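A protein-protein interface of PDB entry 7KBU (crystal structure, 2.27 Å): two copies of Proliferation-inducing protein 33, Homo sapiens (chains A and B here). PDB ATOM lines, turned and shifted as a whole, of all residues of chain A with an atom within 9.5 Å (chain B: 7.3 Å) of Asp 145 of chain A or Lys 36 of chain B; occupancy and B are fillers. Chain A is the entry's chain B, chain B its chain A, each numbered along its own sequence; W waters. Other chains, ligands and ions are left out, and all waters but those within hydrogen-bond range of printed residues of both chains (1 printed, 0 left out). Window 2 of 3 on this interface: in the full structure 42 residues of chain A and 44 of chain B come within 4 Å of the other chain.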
ATOM      1  N   LEU A 105     -13.480   8.633  18.235  1.00  0.00           N
ATOM      2  CA  LEU A 105     -14.812   8.443  18.799  1.00  0.00           C
ATOM      3  C   LEU A 105     -14.775   7.445  19.938  1.00  0.00           C
ATOM      4  O   LEU A 105     -15.453   7.630  20.960  1.00  0.00           O
ATOM      5  CB  LEU A 105     -15.802   8.006  17.712  1.00  0.00           C
ATOM      6  CG  LEU A 105     -16.178   9.120  16.730  1.00  0.00           C
ATOM      7  CD1 LEU A 105     -16.876   8.564  15.507  1.00  0.00           C
ATOM      8  CD2 LEU A 105     -17.051  10.158  17.411  1.00  0.00           C
ATOM      9  N   LEU A 108     -13.479   9.155  22.947  1.00  0.00           N
ATOM     10  CA  LEU A 108     -14.511   9.973  23.578  1.00  0.00           C
ATOM     11  C   LEU A 108     -15.467   9.108  24.390  1.00  0.00           C
ATOM     12  O   LEU A 108     -15.868   9.494  25.491  1.00  0.00           O
ATOM     13  CB  LEU A 108     -15.275  10.792  22.534  1.00  0.00           C
ATOM     14  CG  LEU A 108     -14.433  11.871  21.837  1.00  0.00           C
ATOM     15  CD1 LEU A 108     -15.218  12.581  20.750  1.00  0.00           C
ATOM     16  CD2 LEU A 108     -13.902  12.904  22.832  1.00  0.00           C
ATOM     17  N   GLY A 140     -12.783  19.290  24.491  1.00  0.00           N
ATOM     18  CA  GLY A 140     -13.756  20.364  24.394  1.00  0.00           C
ATOM     19  C   GLY A 140     -14.989  20.137  25.251  1.00  0.00           C
ATOM     20  O   GLY A 140     -15.154  19.076  25.855  1.00  0.00           O
ATOM     21  N   ASP A 141     -15.853  21.153  25.316  1.00  0.00           N
ATOM     22  CA  ASP A 141     -17.076  21.071  26.109  1.00  0.00           C
ATOM     23  C   ASP A 141     -18.185  20.325  25.382  1.00  0.00           C
ATOM     24  O   ASP A 141     -19.079  19.773  26.033  1.00  0.00           O
ATOM     25  CB  ASP A 141     -17.558  22.477  26.468  1.00  0.00           C
ATOM     26  CG  ASP A 141     -16.620  23.193  27.437  1.00  0.00           C
ATOM     27  OD1 ASP A 141     -16.159  22.562  28.418  1.00  0.00           O
ATOM     28  OD2 ASP A 141     -16.350  24.394  27.216  1.00  0.00           O
ATOM     29  N   HIS A 142     -18.132  20.290  24.054  1.00  0.00           N
ATOM     30  CA  HIS A 142     -19.121  19.625  23.212  1.00  0.00           C
ATOM     31  C   HIS A 142     -18.352  18.826  22.179  1.00  0.00           C
ATOM     32  O   HIS A 142     -18.350  19.168  20.994  1.00  0.00           O
ATOM     33  CB  HIS A 142     -20.046  20.623  22.529  1.00  0.00           C
ATOM     34  CG  HIS A 142     -20.642  21.615  23.466  1.00  0.00           C
ATOM     35  ND1 HIS A 142     -21.683  21.302  24.312  1.00  0.00           N
ATOM     36  CD2 HIS A 142     -20.335  22.910  23.706  1.00  0.00           C
ATOM     37  CE1 HIS A 142     -21.999  22.367  25.027  1.00  0.00           C
ATOM     38  NE2 HIS A 142     -21.195  23.357  24.679  1.00  0.00           N
ATOM     39  N   PRO A 143     -17.692  17.746  22.603  1.00  0.00           N
ATOM     40  CA  PRO A 143     -16.707  17.086  21.724  1.00  0.00           C
ATOM     41  C   PRO A 143     -17.256  16.621  20.385  1.00  0.00           C
ATOM     42  O   PRO A 143     -16.606  16.825  19.351  1.00  0.00           O
ATOM     43  CB  PRO A 143     -16.231  15.892  22.576  1.00  0.00           C
ATOM     44  CG  PRO A 143     -16.574  16.252  23.982  1.00  0.00           C
ATOM     45  CD  PRO A 143     -17.808  17.090  23.916  1.00  0.00           C
ATOM     46  N   ILE A 144     -18.420  15.980  20.370  1.00  0.00           N
ATOM     47  CA  ILE A 144     -18.937  15.444  19.112  1.00  0.00           C
ATOM     48  C   ILE A 144     -19.357  16.577  18.189  1.00  0.00           C
ATOM     49  O   ILE A 144     -19.108  16.536  16.978  1.00  0.00           O
ATOM     50  CB  ILE A 144     -20.094  14.475  19.397  1.00  0.00           C
ATOM     51  CG1 ILE A 144     -19.557  13.259  20.143  1.00  0.00           C
ATOM     52  CG2 ILE A 144     -20.782  14.035  18.108  1.00  0.00           C
ATOM     53  CD1 ILE A 144     -18.653  12.393  19.302  1.00  0.00           C
ATOM     54  N   ASP A 145     -20.002  17.604  18.741  1.00  0.00           N
ATOM     55  CA  ASP A 145     -20.358  18.772  17.943  1.00  0.00           C
ATOM     56  C   ASP A 145     -19.118  19.403  17.320  1.00  0.00           C
ATOM     57  O   ASP A 145     -19.123  19.793  16.150  1.00  0.00           O
ATOM     58  CB  ASP A 145     -21.086  19.784  18.817  1.00  0.00           C
ATOM     59  CG  ASP A 145     -21.416  21.050  18.077  1.00  0.00           C
ATOM     60  OD1 ASP A 145     -22.422  21.050  17.329  1.00  0.00           O
ATOM     61  OD2 ASP A 145     -20.667  22.043  18.237  1.00  0.00           O
ATOM     62  N   LEU A 146     -18.053  19.523  18.101  1.00  0.00           N
ATOM     63  CA  LEU A 146     -16.850  20.182  17.629  1.00  0.00           C
ATOM     64  C   LEU A 146     -16.131  19.321  16.610  1.00  0.00           C
ATOM     65  O   LEU A 146     -15.616  19.827  15.607  1.00  0.00           O
ATOM     66  CB  LEU A 146     -15.946  20.479  18.820  1.00  0.00           C
ATOM     67  CG  LEU A 146     -14.659  21.248  18.559  1.00  0.00           C
ATOM     68  CD1 LEU A 146     -14.983  22.613  17.963  1.00  0.00           C
ATOM     69  CD2 LEU A 146     -13.882  21.384  19.865  1.00  0.00           C
ATOM     70  N   LEU A 147     -16.069  18.017  16.868  1.00  0.00           N
ATOM     71  CA  LEU A 147     -15.392  17.114  15.956  1.00  0.00           C
ATOM     72  C   LEU A 147     -16.061  17.102  14.589  1.00  0.00           C
ATOM     73  O   LEU A 147     -15.378  17.186  13.565  1.00  0.00           O
ATOM     74  CB  LEU A 147     -15.371  15.709  16.551  1.00  0.00           C
ATOM     75  CG  LEU A 147     -15.008  14.548  15.625  1.00  0.00           C
ATOM     76  CD1 LEU A 147     -13.523  14.495  15.365  1.00  0.00           C
ATOM     77  CD2 LEU A 147     -15.477  13.248  16.247  1.00  0.00           C
ATOM     78  N   LEU A 148     -17.396  17.085  14.547  1.00  0.00           N
ATOM     79  CA  LEU A 148     -18.052  16.977  13.255  1.00  0.00           C
ATOM     80  C   LEU A 148     -18.098  18.323  12.559  1.00  0.00           C
ATOM     81  O   LEU A 148     -18.057  18.370  11.326  1.00  0.00           O
ATOM     82  CB  LEU A 148     -19.479  16.436  13.398  1.00  0.00           C
ATOM     83  CG  LEU A 148     -19.697  15.105  14.128  1.00  0.00           C
ATOM     84  CD1 LEU A 148     -21.129  14.650  13.909  1.00  0.00           C
ATOM     85  CD2 LEU A 148     -18.710  14.029  13.687  1.00  0.00           C
ATOM     86  N   ARG A 149     -18.183  19.418  13.322  1.00  0.00           N
ATOM     87  CA  ARG A 149     -18.148  20.731  12.693  1.00  0.00           C
ATOM     88  C   ARG A 149     -16.791  20.976  12.044  1.00  0.00           C
ATOM     89  O   ARG A 149     -16.717  21.497  10.928  1.00  0.00           O
ATOM     90  CB  ARG A 149     -18.474  21.822  13.713  1.00  0.00           C
ATOM     91  CG  ARG A 149     -19.937  22.260  13.685  1.00  0.00           C
ATOM     92  CD  ARG A 149     -20.363  22.984  14.970  1.00  0.00           C
ATOM     93  NE  ARG A 149     -20.394  24.439  14.823  1.00  0.00           N
ATOM     94  CZ  ARG A 149     -19.433  25.260  15.230  1.00  0.00           C
ATOM     95  NH1 ARG A 149     -18.330  24.804  15.810  1.00  0.00           N
ATOM     96  NH2 ARG A 149     -19.584  26.574  15.060  1.00  0.00           N
ATOM     97  N   ASP A 150     -15.706  20.609  12.734  1.00  0.00           N
ATOM     98  CA  ASP A 150     -14.370  20.812  12.183  1.00  0.00           C
ATOM     99  C   ASP A 150     -14.120  19.886  10.998  1.00  0.00           C
ATOM    100  O   ASP A 150     -13.497  20.279  10.004  1.00  0.00           O
ATOM    101  CB  ASP A 150     -13.307  20.558  13.258  1.00  0.00           C
ATOM    102  CG  ASP A 150     -13.177  21.705  14.263  1.00  0.00           C
ATOM    103  OD1 ASP A 150     -13.738  22.807  14.046  1.00  0.00           O
ATOM    104  OD2 ASP A 150     -12.495  21.487  15.289  1.00  0.00           O
ATOM    105  N   PHE A 151     -14.574  18.641  11.106  1.00  0.00           N
ATOM    106  CA  PHE A 151     -14.373  17.678  10.032  1.00  0.00           C
ATOM    107  C   PHE A 151     -15.020  18.157   8.742  1.00  0.00           C
ATOM    108  O   PHE A 151     -14.382  18.157   7.681  1.00  0.00           O
ATOM    109  CB  PHE A 151     -14.933  16.326  10.473  1.00  0.00           C
ATOM    110  CG  PHE A 151     -14.626  15.188   9.539  1.00  0.00           C
ATOM    111  CD1 PHE A 151     -15.333  15.029   8.360  1.00  0.00           C
ATOM    112  CD2 PHE A 151     -13.664  14.256   9.865  1.00  0.00           C
ATOM    113  CE1 PHE A 151     -15.068  13.962   7.512  1.00  0.00           C
ATOM    114  CE2 PHE A 151     -13.397  13.196   9.026  1.00  0.00           C
ATOM    115  CZ  PHE A 151     -14.105  13.053   7.844  1.00  0.00           C
ATOM    116  N   LYS A 152     -16.274  18.610   8.818  1.00  0.00           N
ATOM    117  CA  LYS A 152     -17.009  19.051   7.637  1.00  0.00           C
ATOM    118  C   LYS A 152     -16.487  20.359   7.060  1.00  0.00           C
ATOM    119  O   LYS A 152     -16.869  20.716   5.937  1.00  0.00           O
ATOM    120  CB  LYS A 152     -18.505  19.170   7.972  1.00  0.00           C
ATOM    121  CG  LYS A 152     -19.139  17.776   8.180  1.00  0.00           C
ATOM    122  CD  LYS A 152     -20.625  17.744   7.885  1.00  0.00           C
ATOM    123  CE  LYS A 152     -21.150  16.338   8.107  1.00  0.00           C
ATOM    124  NZ  LYS A 152     -22.624  16.272   8.200  1.00  0.00           N
ATOM    125  N   LYS A 153     -15.662  21.096   7.805  1.00  0.00           N
ATOM    126  CA  LYS A 153     -14.967  22.262   7.281  1.00  0.00           C
ATOM    127  C   LYS A 153     -13.606  21.913   6.691  1.00  0.00           C
ATOM    128  O   LYS A 153     -12.979  22.776   6.071  1.00  0.00           O
ATOM    129  CB  LYS A 153     -14.804  23.338   8.373  1.00  0.00           C
ATOM    130  CG  LYS A 153     -16.104  24.106   8.652  1.00  0.00           C
ATOM    131  CD  LYS A 153     -15.922  25.431   9.392  1.00  0.00           C
ATOM    132  CE  LYS A 153     -15.071  26.471   8.621  1.00  0.00           C
ATOM    133  NZ  LYS A 153     -15.860  27.276   7.611  1.00  0.00           N
ATOM    134  N   LYS A 224     -20.728  24.932   4.410  1.00  0.00           N
ATOM    135  CA  LYS A 224     -21.062  26.351   4.420  1.00  0.00           C
ATOM    136  C   LYS A 224     -20.910  26.965   3.025  1.00  0.00           C
ATOM    137  O   LYS A 224     -20.102  26.513   2.197  1.00  0.00           O
ATOM    138  CB  LYS A 224     -20.175  27.097   5.417  1.00  0.00           C
ATOM    139  CG  LYS A 224     -20.274  26.570   6.835  1.00  0.00           C
ATOM    140  CD  LYS A 224     -21.721  26.620   7.351  1.00  0.00           C
ATOM    141  CE  LYS A 224     -21.835  26.114   8.789  1.00  0.00           C
ATOM    142  NZ  LYS A 224     -22.869  25.033   8.954  1.00  0.00           N
ATOM    143  N   PRO B  33     -23.962  21.178  31.978  1.00  0.00           N
ATOM    144  CA  PRO B  33     -23.730  22.260  31.000  1.00  0.00           C
ATOM    145  C   PRO B  33     -24.833  22.316  29.959  1.00  0.00           C
ATOM    146  O   PRO B  33     -25.432  21.286  29.621  1.00  0.00           O
ATOM    147  CB  PRO B  33     -22.386  21.878  30.354  1.00  0.00           C
ATOM    148  CG  PRO B  33     -21.711  20.971  31.332  1.00  0.00           C
ATOM    149  CD  PRO B  33     -22.803  20.271  32.105  1.00  0.00           C
ATOM    150  N   PRO B  34     -25.121  23.496  29.405  1.00  0.00           N
ATOM    151  CA  PRO B  34     -26.084  23.563  28.298  1.00  0.00           C
ATOM    152  C   PRO B  34     -25.623  22.696  27.134  1.00  0.00           C
ATOM    153  O   PRO B  34     -24.431  22.441  26.952  1.00  0.00           O
ATOM    154  CB  PRO B  34     -26.108  25.052  27.930  1.00  0.00           C
ATOM    155  CG  PRO B  34     -25.607  25.754  29.132  1.00  0.00           C
ATOM    156  CD  PRO B  34     -24.613  24.831  29.770  1.00  0.00           C
ATOM    157  N   THR B  35     -26.585  22.227  26.351  1.00  0.00           N
ATOM    158  CA  THR B  35     -26.340  21.202  25.353  1.00  0.00           C
ATOM    159  C   THR B  35     -26.637  21.715  23.950  1.00  0.00           C
ATOM    160  O   THR B  35     -27.509  22.565  23.744  1.00  0.00           O
ATOM    161  CB  THR B  35     -27.190  19.944  25.613  1.00  0.00           C
ATOM    162  OG1 THR B  35     -28.582  20.274  25.514  1.00  0.00           O
ATOM    163  CG2 THR B  35     -26.891  19.355  26.987  1.00  0.00           C
ATOM    164  N   LYS B  36     -25.855  21.228  23.004  1.00  0.00           N
ATOM    165  CA  LYS B  36     -26.109  21.369  21.582  1.00  0.00           C
ATOM    166  C   LYS B  36     -26.726  20.079  21.053  1.00  0.00           C
ATOM    167  O   LYS B  36     -26.532  19.005  21.629  1.00  0.00           O
ATOM    168  CB  LYS B  36     -24.801  21.688  20.851  1.00  0.00           C
ATOM    169  CG  LYS B  36     -24.112  22.950  21.363  1.00  0.00           C
ATOM    170  CD  LYS B  36     -22.748  23.171  20.715  1.00  0.00           C
ATOM    171  CE  LYS B  36     -22.758  24.365  19.739  1.00  0.00           C
ATOM    172  NZ  LYS B  36     -22.943  23.978  18.290  1.00  0.00           N
ATOM    173  N   PRO B  37     -27.480  20.139  19.954  1.00  0.00           N
ATOM    174  CA  PRO B  37     -28.074  18.902  19.409  1.00  0.00           C
ATOM    175  C   PRO B  37     -27.122  17.720  19.304  1.00  0.00           C
ATOM    176  O   PRO B  37     -27.487  16.599  19.677  1.00  0.00           O
ATOM    177  CB  PRO B  37     -28.561  19.350  18.025  1.00  0.00           C
ATOM    178  CG  PRO B  37     -28.861  20.814  18.176  1.00  0.00           C
ATOM    179  CD  PRO B  37     -28.021  21.352  19.308  1.00  0.00           C
ATOM    180  N   LEU B  38     -25.904  17.932  18.833  1.00  0.00           N
ATOM    181  CA  LEU B  38     -24.997  16.816  18.600  1.00  0.00           C
ATOM    182  C   LEU B  38     -24.400  16.241  19.876  1.00  0.00           C
ATOM    183  O   LEU B  38     -23.658  15.254  19.787  1.00  0.00           O
ATOM    184  CB  LEU B  38     -23.889  17.252  17.644  1.00  0.00           C
ATOM    185  CG  LEU B  38     -24.347  17.316  16.185  1.00  0.00           C
ATOM    186  CD1 LEU B  38     -23.304  18.032  15.348  1.00  0.00           C
ATOM    187  CD2 LEU B  38     -24.610  15.909  15.656  1.00  0.00           C
ATOM    188  N   ASP B  39     -24.699  16.825  21.047  1.00  0.00           N
ATOM    189  CA  ASP B  39     -24.292  16.238  22.317  1.00  0.00           C
ATOM    190  C   ASP B  39     -25.177  15.064  22.720  1.00  0.00           C
ATOM    191  O   ASP B  39     -24.806  14.298  23.622  1.00  0.00           O
ATOM    192  CB  ASP B  39     -24.358  17.283  23.444  1.00  0.00           C
ATOM    193  CG  ASP B  39     -23.317  18.386  23.303  1.00  0.00           C
ATOM    194  OD1 ASP B  39     -22.207  18.118  22.789  1.00  0.00           O
ATOM    195  OD2 ASP B  39     -23.617  19.526  23.729  1.00  0.00           O
ATOM    196  N   GLN B  40     -26.312  14.902  22.057  1.00  0.00           N
ATOM    197  CA  GLN B  40     -27.268  13.877  22.444  1.00  0.00           C
ATOM    198  C   GLN B  40     -26.621  12.504  22.379  1.00  0.00           C
ATOM    199  O   GLN B  40     -25.714  12.256  21.578  1.00  0.00           O
ATOM    200  CB  GLN B  40     -28.489  13.914  21.528  1.00  0.00           C
ATOM    201  CG  GLN B  40     -29.584  14.832  21.988  1.00  0.00           C
ATOM    202  CD  GLN B  40     -30.492  15.264  20.855  1.00  0.00           C
ATOM    203  OE1 GLN B  40     -30.516  14.648  19.793  1.00  0.00           O
ATOM    204  NE2 GLN B  40     -31.251  16.330  21.081  1.00  0.00           N
ATOM    205  N   ALA B  50     -30.050  14.409  26.679  1.00  0.00           N
ATOM    206  CA  ALA B  50     -29.556  15.640  26.071  1.00  0.00           C
ATOM    207  C   ALA B  50     -28.045  15.622  25.965  1.00  0.00           C
ATOM    208  O   ALA B  50     -27.467  16.198  25.031  1.00  0.00           O
ATOM    209  CB  ALA B  50     -29.983  16.865  26.892  1.00  0.00           C
ATOM    210  N   SER B  51     -27.393  14.962  26.910  1.00  0.00           N
ATOM    211  CA  SER B  51     -25.962  14.767  26.839  1.00  0.00           C
ATOM    212  C   SER B  51     -25.565  13.634  27.774  1.00  0.00           C
ATOM    213  O   SER B  51     -26.374  13.094  28.540  1.00  0.00           O
ATOM    214  CB  SER B  51     -25.215  16.041  27.216  1.00  0.00           C
ATOM    215  OG  SER B  51     -25.101  16.127  28.623  1.00  0.00           O
HETATM  216  O   HOH W   1     -20.620  16.302  22.169  1.00  0.00           O
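OD2 of Asp 145 of chain A is in salt-bridge range of NZ of Lys 36 of chain B (3.0 Å).
ND1 of His 142 of chain A lies within hydrogen-bond range of OD2 of Asp 39 of chain B, at 2.7 Å.
The backbone NH (N) of Lys 36 of chain B is in hydrogen-bond range of the side-chain carboxylate (OD2) of Asp 39 of chain B.
Among the printed residues, pairs that only touch across the chains: His 142 of chain A with Pro 34 of chain B, Ile 144 of chain A with Leu 38 of chain B, Asp 145 of chain A with Leu 38 of chain B and His 142 of chain A with Lys 36 of chain B.
Of chain B, only Lys 36 and Leu 38 come within 4 Å of Asp 145 of chain A.
Of the printed residues of chain A, Lys 36 of chain B touches His 142 and Asp 145.
No residue of chain A comes within 4 Å of Thr 35 of chain B.
No residue of chain A comes within 4 Å of Pro 37 of chain B.
Asp 39 of chain B touches just one residue of chain A: His 142 (2.7 Å).
Of the printed residues of chain B, Ile 144 of chain A touches Leu 38.
Printed residues of chain A within 4 Å of Pro 34 of chain B: His 142.
Printed residues of chain B within 4 Å of His 142 of chain A: Pro 34 (3.1 Å), Lys 36 (3.8 Å) and Asp 39 (2.7 Å).
Printed residues of chain A within 4 Å of Leu 38 of chain B: Ile 144 (3.5 Å) and Asp 145 (3.7 Å).
Leu 147 of chain A touches none of the printed residues of chain B.
Gly 140 of chain A touches none of the printed residues of chain B.
The nearest residue of chain B that does not touch Asp 145 of chain A is Asp 39 of chain B (4.5 Å).
The nearest residue of chain A that does not touch Lys 36 of chain B is Arg 149 of chain A (4.3 Å).
The nearest printed residue of chain B that does not touch Ile 144 of chain A is Asp 39 of chain B (5.0 Å).
Of the 10 printed residues of chain B, 4 touch a printed residue of chain A.
Hydrophobic or aromatic side chains of chain B within 4 Å of the printed part of chain A: Leu 38.
Along chain A the printed residues that touch a printed residue of chain B span positions 142 to 145.
Among the printed residues, 6 pairs touch across the chains.
Among the printed residues, Asp or Glu carboxylates within 4 Å of a Lys or Arg side-chain nitrogen of the other chain: Asp 145 of chain A with Lys 36 of chain B.
No position is printed for both chains.
Water W1 bridges OD1 of Asp 39 of chain B (2.5 Å) and N of Ile 144 of chain A (2.9 Å).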
